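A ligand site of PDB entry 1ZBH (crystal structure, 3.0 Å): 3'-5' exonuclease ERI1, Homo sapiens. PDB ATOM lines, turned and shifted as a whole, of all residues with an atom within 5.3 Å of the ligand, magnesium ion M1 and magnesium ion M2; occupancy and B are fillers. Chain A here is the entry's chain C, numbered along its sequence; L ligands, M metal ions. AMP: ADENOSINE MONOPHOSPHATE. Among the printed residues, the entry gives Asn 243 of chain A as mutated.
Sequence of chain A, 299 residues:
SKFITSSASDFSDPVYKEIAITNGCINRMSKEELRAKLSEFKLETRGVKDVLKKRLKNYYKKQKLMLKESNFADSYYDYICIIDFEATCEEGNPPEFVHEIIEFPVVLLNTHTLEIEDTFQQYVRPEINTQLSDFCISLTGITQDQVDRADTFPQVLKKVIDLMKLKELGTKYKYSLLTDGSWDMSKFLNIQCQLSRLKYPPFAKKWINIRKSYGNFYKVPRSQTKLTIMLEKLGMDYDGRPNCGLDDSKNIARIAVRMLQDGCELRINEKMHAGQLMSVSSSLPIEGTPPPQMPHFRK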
ATOM      1  N   ASP A  84      11.150  18.942  -7.385  1.00  0.00           N
ATOM      2  CA  ASP A  84      11.107  17.509  -7.630  1.00  0.00           C
ATOM      3  C   ASP A  84       9.984  16.893  -6.822  1.00  0.00           C
ATOM      4  O   ASP A  84      10.151  16.575  -5.644  1.00  0.00           O
ATOM      5  CB  ASP A  84      12.438  16.836  -7.288  1.00  0.00           C
ATOM      6  CG  ASP A  84      12.459  15.366  -7.665  1.00  0.00           C
ATOM      7  OD1 ASP A  84      12.287  15.054  -8.865  1.00  0.00           O
ATOM      8  OD2 ASP A  84      12.638  14.516  -6.768  1.00  0.00           O
ATOM      9  N   PHE A  85       8.822  16.727  -7.459  1.00  0.00           N
ATOM     10  CA  PHE A  85       7.692  16.078  -6.822  1.00  0.00           C
ATOM     11  C   PHE A  85       8.000  14.623  -6.489  1.00  0.00           C
ATOM     12  O   PHE A  85       8.697  13.940  -7.255  1.00  0.00           O
ATOM     13  CB  PHE A  85       6.453  16.135  -7.714  1.00  0.00           C
ATOM     14  CG  PHE A  85       5.909  17.511  -7.928  1.00  0.00           C
ATOM     15  CD1 PHE A  85       5.497  18.289  -6.844  1.00  0.00           C
ATOM     16  CD2 PHE A  85       5.772  18.019  -9.206  1.00  0.00           C
ATOM     17  CE1 PHE A  85       4.987  19.555  -7.045  1.00  0.00           C
ATOM     18  CE2 PHE A  85       5.259  19.284  -9.421  1.00  0.00           C
ATOM     19  CZ  PHE A  85       4.863  20.059  -8.326  1.00  0.00           C
ATOM     20  N   GLU A  86       7.491  14.171  -5.355  1.00  0.00           N
ATOM     21  CA  GLU A  86       7.329  12.747  -5.103  1.00  0.00           C
ATOM     22  C   GLU A  86       5.828  12.444  -5.147  1.00  0.00           C
ATOM     23  O   GLU A  86       5.008  13.259  -4.732  1.00  0.00           O
ATOM     24  CB  GLU A  86       7.934  12.331  -3.763  1.00  0.00           C
ATOM     25  CG  GLU A  86       9.444  12.534  -3.651  1.00  0.00           C
ATOM     26  CD  GLU A  86      10.236  11.899  -4.796  1.00  0.00           C
ATOM     27  OE1 GLU A  86       9.989  10.722  -5.130  1.00  0.00           O
ATOM     28  OE2 GLU A  86      11.121  12.581  -5.362  1.00  0.00           O
ATOM     29  N   ALA A  87       5.484  11.273  -5.672  1.00  0.00           N
ATOM     30  CA  ALA A  87       4.088  10.920  -5.892  1.00  0.00           C
ATOM     31  C   ALA A  87       3.815   9.483  -5.490  1.00  0.00           C
ATOM     32  O   ALA A  87       4.732   8.667  -5.419  1.00  0.00           O
ATOM     33  CB  ALA A  87       3.716  11.147  -7.359  1.00  0.00           C
ATOM     34  N   THR A  88       2.552   9.183  -5.225  1.00  0.00           N
ATOM     35  CA  THR A  88       2.096   7.814  -5.001  1.00  0.00           C
ATOM     36  C   THR A  88       2.542   6.947  -6.188  1.00  0.00           C
ATOM     37  O   THR A  88       2.626   7.437  -7.311  1.00  0.00           O
ATOM     38  CB  THR A  88       0.565   7.741  -4.863  1.00  0.00           C
ATOM     39  OG1 THR A  88      -0.055   8.331  -6.021  1.00  0.00           O
ATOM     40  CG2 THR A  88       0.087   8.466  -3.614  1.00  0.00           C
ATOM     41  N   CYS A  89       2.832   5.676  -5.925  1.00  0.00           N
ATOM     42  CA  CYS A  89       3.308   4.782  -6.986  1.00  0.00           C
ATOM     43  C   CYS A  89       3.141   3.305  -6.638  1.00  0.00           C
ATOM     44  O   CYS A  89       2.659   2.966  -5.549  1.00  0.00           O
ATOM     45  CB  CYS A  89       4.778   5.051  -7.287  1.00  0.00           C
ATOM     46  SG  CYS A  89       5.827   5.005  -5.836  1.00  0.00           S
ATOM     47  N   GLU A  90       3.544   2.450  -7.572  1.00  0.00           N
ATOM     48  CA  GLU A  90       3.374   1.017  -7.434  1.00  0.00           C
ATOM     49  C   GLU A  90       4.488   0.270  -8.172  1.00  0.00           C
ATOM     50  O   GLU A  90       4.995   0.754  -9.192  1.00  0.00           O
ATOM     51  CB  GLU A  90       2.016   0.614  -8.010  1.00  0.00           C
ATOM     52  CG  GLU A  90       1.195  -0.258  -7.095  1.00  0.00           C
ATOM     53  CD  GLU A  90      -0.299  -0.062  -7.307  1.00  0.00           C
ATOM     54  OE1 GLU A  90      -0.977   0.346  -6.338  1.00  0.00           O
ATOM     55  OE2 GLU A  90      -0.787  -0.304  -8.430  1.00  0.00           O
ATOM     56  N   GLY A  92       6.743  -1.803 -10.548  1.00  0.00           N
ATOM     57  CA  GLY A  92       6.683  -1.936 -11.998  1.00  0.00           C
ATOM     58  C   GLY A  92       6.336  -0.639 -12.713  1.00  0.00           C
ATOM     59  O   GLY A  92       6.516  -0.540 -13.922  1.00  0.00           O
ATOM     60  N   ASN A  93       5.852   0.334 -11.948  1.00  0.00           N
ATOM     61  CA  ASN A  93       5.473   1.656 -12.456  1.00  0.00           C
ATOM     62  C   ASN A  93       4.462   1.626 -13.616  1.00  0.00           C
ATOM     63  O   ASN A  93       4.771   2.129 -14.702  1.00  0.00           O
ATOM     64  CB  ASN A  93       6.734   2.451 -12.844  1.00  0.00           C
ATOM     65  CG  ASN A  93       6.516   3.967 -12.822  1.00  0.00           C
ATOM     66  OD1 ASN A  93       7.450   4.726 -12.609  1.00  0.00           O
ATOM     67  ND2 ASN A  93       5.277   4.401 -13.054  1.00  0.00           N
ATOM     68  N   HIS A  99      -1.153   9.186 -10.615  1.00  0.00           N
ATOM     69  CA  HIS A  99      -0.222   9.676  -9.598  1.00  0.00           C
ATOM     70  C   HIS A  99      -0.795  10.837  -8.804  1.00  0.00           C
ATOM     71  O   HIS A  99      -1.504  11.687  -9.346  1.00  0.00           O
ATOM     72  CB  HIS A  99       1.099  10.106 -10.224  1.00  0.00           C
ATOM     73  CG  HIS A  99       1.854   8.977 -10.866  1.00  0.00           C
ATOM     74  ND1 HIS A  99       2.658   8.121 -10.146  1.00  0.00           N
ATOM     75  CD2 HIS A  99       1.935   8.588 -12.158  1.00  0.00           C
ATOM     76  CE1 HIS A  99       3.200   7.242 -10.968  1.00  0.00           C
ATOM     77  NE2 HIS A  99       2.774   7.502 -12.197  1.00  0.00           N
ATOM     78  N   PHE A 135       5.650  -0.221  -1.354  1.00  0.00           N
ATOM     79  CA  PHE A 135       6.656   0.117  -2.358  1.00  0.00           C
ATOM     80  C   PHE A 135       6.944   1.624  -2.385  1.00  0.00           C
ATOM     81  O   PHE A 135       8.094   2.034  -2.519  1.00  0.00           O
ATOM     82  CB  PHE A 135       6.271  -0.379  -3.755  1.00  0.00           C
ATOM     83  CG  PHE A 135       7.277  -0.036  -4.810  1.00  0.00           C
ATOM     84  CD1 PHE A 135       8.511  -0.679  -4.862  1.00  0.00           C
ATOM     85  CD2 PHE A 135       6.996   0.946  -5.760  1.00  0.00           C
ATOM     86  CE1 PHE A 135       9.458  -0.357  -5.840  1.00  0.00           C
ATOM     87  CE2 PHE A 135       7.927   1.272  -6.749  1.00  0.00           C
ATOM     88  CZ  PHE A 135       9.162   0.619  -6.787  1.00  0.00           C
ATOM     89  N   LEU A 139      10.498   3.400  -1.457  1.00  0.00           N
ATOM     90  CA  LEU A 139      11.214   4.176  -2.456  1.00  0.00           C
ATOM     91  C   LEU A 139      11.483   5.615  -2.023  1.00  0.00           C
ATOM     92  O   LEU A 139      12.636   6.049  -2.001  1.00  0.00           O
ATOM     93  CB  LEU A 139      10.466   4.172  -3.802  1.00  0.00           C
ATOM     94  CG  LEU A 139      11.109   4.985  -4.934  1.00  0.00           C
ATOM     95  CD1 LEU A 139      12.381   4.324  -5.438  1.00  0.00           C
ATOM     96  CD2 LEU A 139      10.120   5.199  -6.065  1.00  0.00           C
ATOM     97  N   THR A 140      10.420   6.326  -1.674  1.00  0.00           N
ATOM     98  CA  THR A 140      10.495   7.758  -1.370  1.00  0.00           C
ATOM     99  C   THR A 140      10.944   8.046   0.060  1.00  0.00           C
ATOM    100  O   THR A 140      11.498   9.105   0.336  1.00  0.00           O
ATOM    101  CB  THR A 140       9.143   8.445  -1.594  1.00  0.00           C
ATOM    102  OG1 THR A 140       8.164   7.841  -0.741  1.00  0.00           O
ATOM    103  CG2 THR A 140       8.720   8.304  -3.043  1.00  0.00           C
ATOM    104  N   ASP A 180      13.879  17.748 -13.059  1.00  0.00           N
ATOM    105  CA  ASP A 180      14.714  16.647 -13.529  1.00  0.00           C
ATOM    106  C   ASP A 180      13.878  15.734 -14.415  1.00  0.00           C
ATOM    107  O   ASP A 180      13.398  14.680 -13.964  1.00  0.00           O
ATOM    108  CB  ASP A 180      15.294  15.873 -12.341  1.00  0.00           C
ATOM    109  CG  ASP A 180      16.210  14.746 -12.774  1.00  0.00           C
ATOM    110  OD1 ASP A 180      16.883  14.900 -13.810  1.00  0.00           O
ATOM    111  OD2 ASP A 180      16.246  13.705 -12.087  1.00  0.00           O
ATOM    112  N   TRP A 183       8.142  14.802 -16.588  1.00  0.00           N
ATOM    113  CA  TRP A 183       6.975  14.294 -15.849  1.00  0.00           C
ATOM    114  C   TRP A 183       6.539  15.178 -14.672  1.00  0.00           C
ATOM    115  O   TRP A 183       5.343  15.393 -14.464  1.00  0.00           O
ATOM    116  CB  TRP A 183       7.192  12.839 -15.406  1.00  0.00           C
ATOM    117  CG  TRP A 183       8.605  12.556 -14.982  1.00  0.00           C
ATOM    118  CD1 TRP A 183       9.133  12.647 -13.708  1.00  0.00           C
ATOM    119  CD2 TRP A 183       9.681  12.149 -15.829  1.00  0.00           C
ATOM    120  NE1 TRP A 183      10.469  12.324 -13.721  1.00  0.00           N
ATOM    121  CE2 TRP A 183      10.835  12.012 -15.011  1.00  0.00           C
ATOM    122  CE3 TRP A 183       9.794  11.889 -17.205  1.00  0.00           C
ATOM    123  CZ2 TRP A 183      12.084  11.625 -15.524  1.00  0.00           C
ATOM    124  CZ3 TRP A 183      11.037  11.512 -17.724  1.00  0.00           C
ATOM    125  CH2 TRP A 183      12.168  11.374 -16.873  1.00  0.00           C
ATOM    126  N   ASP A 184       7.496  15.681 -13.912  1.00  0.00           N
ATOM    127  CA  ASP A 184       7.201  16.520 -12.752  1.00  0.00           C
ATOM    128  C   ASP A 184       6.113  17.543 -13.039  1.00  0.00           C
ATOM    129  O   ASP A 184       5.129  17.651 -12.303  1.00  0.00           O
ATOM    130  CB  ASP A 184       8.464  17.208 -12.236  1.00  0.00           C
ATOM    131  CG  ASP A 184       9.398  16.259 -11.529  1.00  0.00           C
ATOM    132  OD1 ASP A 184      10.434  15.872 -12.125  1.00  0.00           O
ATOM    133  OD2 ASP A 184       9.095  15.874 -10.370  1.00  0.00           O
ATOM    134  N   PHE A 188       2.828  14.984 -13.247  1.00  0.00           N
ATOM    135  CA  PHE A 188       2.455  15.039 -11.836  1.00  0.00           C
ATOM    136  C   PHE A 188       1.572  16.240 -11.534  1.00  0.00           C
ATOM    137  O   PHE A 188       0.436  16.069 -11.104  1.00  0.00           O
ATOM    138  CB  PHE A 188       3.703  15.012 -10.932  1.00  0.00           C
ATOM    139  CG  PHE A 188       4.458  13.709 -10.976  1.00  0.00           C
ATOM    140  CD1 PHE A 188       3.800  12.502 -11.212  1.00  0.00           C
ATOM    141  CD2 PHE A 188       5.835  13.685 -10.751  1.00  0.00           C
ATOM    142  CE1 PHE A 188       4.500  11.295 -11.242  1.00  0.00           C
ATOM    143  CE2 PHE A 188       6.534  12.478 -10.781  1.00  0.00           C
ATOM    144  CZ  PHE A 188       5.871  11.283 -11.024  1.00  0.00           C
ATOM    145  N   ARG A 211      17.600  17.270 -17.680  1.00  0.00           N
ATOM    146  CA  ARG A 211      18.052  16.118 -18.459  1.00  0.00           C
ATOM    147  C   ARG A 211      18.222  16.497 -19.917  1.00  0.00           C
ATOM    148  O   ARG A 211      19.177  16.063 -20.568  1.00  0.00           O
ATOM    149  CB  ARG A 211      17.088  14.942 -18.331  1.00  0.00           C
ATOM    150  CG  ARG A 211      17.148  14.231 -16.994  1.00  0.00           C
ATOM    151  CD  ARG A 211      15.923  13.368 -16.812  1.00  0.00           C
ATOM    152  NE  ARG A 211      15.821  12.873 -15.440  1.00  0.00           N
ATOM    153  CZ  ARG A 211      15.945  11.586 -15.088  1.00  0.00           C
ATOM    154  NH1 ARG A 211      16.148  10.655 -16.005  1.00  0.00           N
ATOM    155  NH2 ARG A 211      15.847  11.257 -13.804  1.00  0.00           N
ATOM    156  N   ASN A 243      15.541   9.803  -3.640  1.00  0.00           N
ATOM    157  CA  ASN A 243      14.067   9.817  -3.768  1.00  0.00           C
ATOM    158  C   ASN A 243      13.298  10.496  -2.644  1.00  0.00           C
ATOM    159  O   ASN A 243      12.071  10.457  -2.591  1.00  0.00           O
ATOM    160  CB  ASN A 243      13.520   8.423  -4.081  1.00  0.00           C
ATOM    161  CG  ASN A 243      13.897   7.956  -5.474  1.00  0.00           C
ATOM    162  OD1 ASN A 243      13.413   8.508  -6.468  1.00  0.00           O
ATOM    163  ND2 ASN A 243      14.764   6.953  -5.551  1.00  0.00           N
ATOM    164  N   CYS A 244      14.033  11.136  -1.734  1.00  0.00           N
ATOM    165  CA  CYS A 244      13.459  12.122  -0.825  1.00  0.00           C
ATOM    166  C   CYS A 244      13.458  13.425  -1.602  1.00  0.00           C
ATOM    167  O   CYS A 244      14.500  14.041  -1.798  1.00  0.00           O
ATOM    168  CB  CYS A 244      14.316  12.229   0.446  1.00  0.00           C
ATOM    169  SG  CYS A 244      14.162  13.752   1.435  1.00  0.00           S
ATOM    170  N   GLY A 245      12.275  13.835  -2.074  1.00  0.00           N
ATOM    171  CA  GLY A 245      12.112  14.990  -2.974  1.00  0.00           C
ATOM    172  C   GLY A 245      13.044  16.174  -2.743  1.00  0.00           C
ATOM    173  O   GLY A 245      13.634  16.705  -3.695  1.00  0.00           O
ATOM    174  N   ASP A 248      16.613  15.166  -3.686  1.00  0.00           N
ATOM    175  CA  ASP A 248      16.773  15.146  -5.139  1.00  0.00           C
ATOM    176  C   ASP A 248      16.915  16.560  -5.674  1.00  0.00           C
ATOM    177  O   ASP A 248      17.800  16.841  -6.474  1.00  0.00           O
ATOM    178  CB  ASP A 248      15.631  14.414  -5.834  1.00  0.00           C
ATOM    179  CG  ASP A 248      15.507  12.975  -5.416  1.00  0.00           C
ATOM    180  OD1 ASP A 248      14.966  12.722  -4.328  1.00  0.00           O
ATOM    181  OD2 ASP A 248      15.948  12.085  -6.169  1.00  0.00           O
HETATM  182  P   AMP L   1      11.789  10.949  -9.404  1.00  0.00           P
HETATM  183  O1P AMP L   1      11.758  12.372  -8.886  1.00  0.00           O
HETATM  184  O2P AMP L   1      12.954  10.132  -8.917  1.00  0.00           O
HETATM  185  O3P AMP L   1      11.507  10.834 -10.887  1.00  0.00           O
HETATM  186  O5' AMP L   1      10.536  10.220  -8.718  1.00  0.00           O
HETATM  187  C5' AMP L   1       9.304  10.904  -8.539  1.00  0.00           C
HETATM  188  C4' AMP L   1       8.128   9.946  -8.497  1.00  0.00           C
HETATM  189  O4' AMP L   1       8.120   9.105  -9.653  1.00  0.00           O
HETATM  190  C3' AMP L   1       8.169   8.998  -7.312  1.00  0.00           C
HETATM  191  O3' AMP L   1       7.567   9.580  -6.149  1.00  0.00           O
HETATM  192  C2' AMP L   1       7.401   7.795  -7.809  1.00  0.00           C
HETATM  193  O2' AMP L   1       5.996   7.954  -7.617  1.00  0.00           O
HETATM  194  C1' AMP L   1       7.690   7.783  -9.299  1.00  0.00           C
HETATM  195  N9  AMP L   1       8.777   6.791  -9.489  1.00  0.00           N
HETATM  196  C8  AMP L   1      10.091   7.060  -9.625  1.00  0.00           C
HETATM  197  N7  AMP L   1      10.818   5.920  -9.764  1.00  0.00           N
HETATM  198  C5  AMP L   1       9.952   4.890  -9.705  1.00  0.00           C
HETATM  199  C6  AMP L   1      10.046   3.409  -9.771  1.00  0.00           C
HETATM  200  N6  AMP L   1      11.248   2.805  -9.941  1.00  0.00           N
HETATM  201  N1  AMP L   1       8.912   2.694  -9.662  1.00  0.00           N
HETATM  202  C2  AMP L   1       7.713   3.287  -9.499  1.00  0.00           C
HETATM  203  N3  AMP L   1       7.548   4.621  -9.420  1.00  0.00           N
HETATM  204  C4  AMP L   1       8.612   5.466  -9.522  1.00  0.00           C
HETATM  205 MG    MG M   1      11.994  13.643 -10.345  1.00  0.00          MG
HETATM  206 MG    MG M   2      12.771  12.386  -6.611  1.00  0.00          MG
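O2P of the ligand sits close to OD1 of Asn 243 (3.0 Å). The side-chain sulfur (SG) of Cys 89 lies close to an oxygen (O2') of the ligand, at 3.4 Å. The side-chain amide oxygen (OD1) of Asn 93 sits close to a nitrogen (N3) of the ligand (3.2 Å). The indole nitrogen (NE1) of Trp 183 is in hydrogen-bond range of an oxygen (O3P) of the ligand (3.4 Å). The backbone NH (N) of Ala 87 is in hydrogen-bond range of an oxygen (O3') of the ligand, 2.7 Å away. The backbone carbonyl oxygen (O) of Ala 87 sits at hydrogen-bond distance from an oxygen (O2') of the ligand. O of Thr 88 is in hydrogen-bond range of O2' of the ligand (3.4 Å).
The backbone carbonyl oxygen (O) of Trp 183 sits at hydrogen-bond distance from the backbone NH (N) of Phe 188. The side-chain carboxylate of Asp 248 sits at hydrogen-bond distance from the backbone NH of Asn 243 (3.1 Å). The side-chain carboxylate (OD2) of Asp 184 is in hydrogen-bond range of the backbone NH (N) of Phe 85, 3.0 Å away. The backbone carbonyl oxygen of Thr 88 sits at hydrogen-bond distance from a ring nitrogen (ND1) of His 99, 2.9 Å away. The side-chain carboxylate (OD1) of Asp 248 is in hydrogen-bond range of the backbone NH (N) of Cys 244 (3.2 Å).
Residues that only touch the ligand: Phe 85, Phe 135, Phe 188, Thr 140, Leu 139 and Glu 90. Hydrophobic or aromatic side chains that line the ligand: Ala 87, Phe 135, Leu 139 and Phe 188. Of the 22 residues printed, 14 come within 4 Å of the ligand. The nearest printed residue that does not touch the ligand is His 99 (4.2 Å).
Merely in contact with magnesium ion M1: Asp 184 (3.3 Å) and Trp 183 (3.9 Å). Within 4 Å of magnesium ion M1: Asp 84, Trp 183 and Asp 184. Along chain A the residues within 4 Å of magnesium ion M1 span positions 84 to 184.
OD1 of Asn 243 touches magnesium ion M2, 3.9 Å away. Asp 248 touches magnesium ion M2.
Magnesium ion M1 is bound by O1P of the ligand (1.9 Å) and OD1 of Asp 84 (2.1 Å).
OE2 of Glu 86 binds magnesium ion M2, 2.1 Å away. Magnesium ion M2 is bound by the side-chain carboxylate (OD2) of Asp 84, at 2.1 Å. An oxygen (O1P) of the ligand is bound to magnesium ion M2 (2.5 Å).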
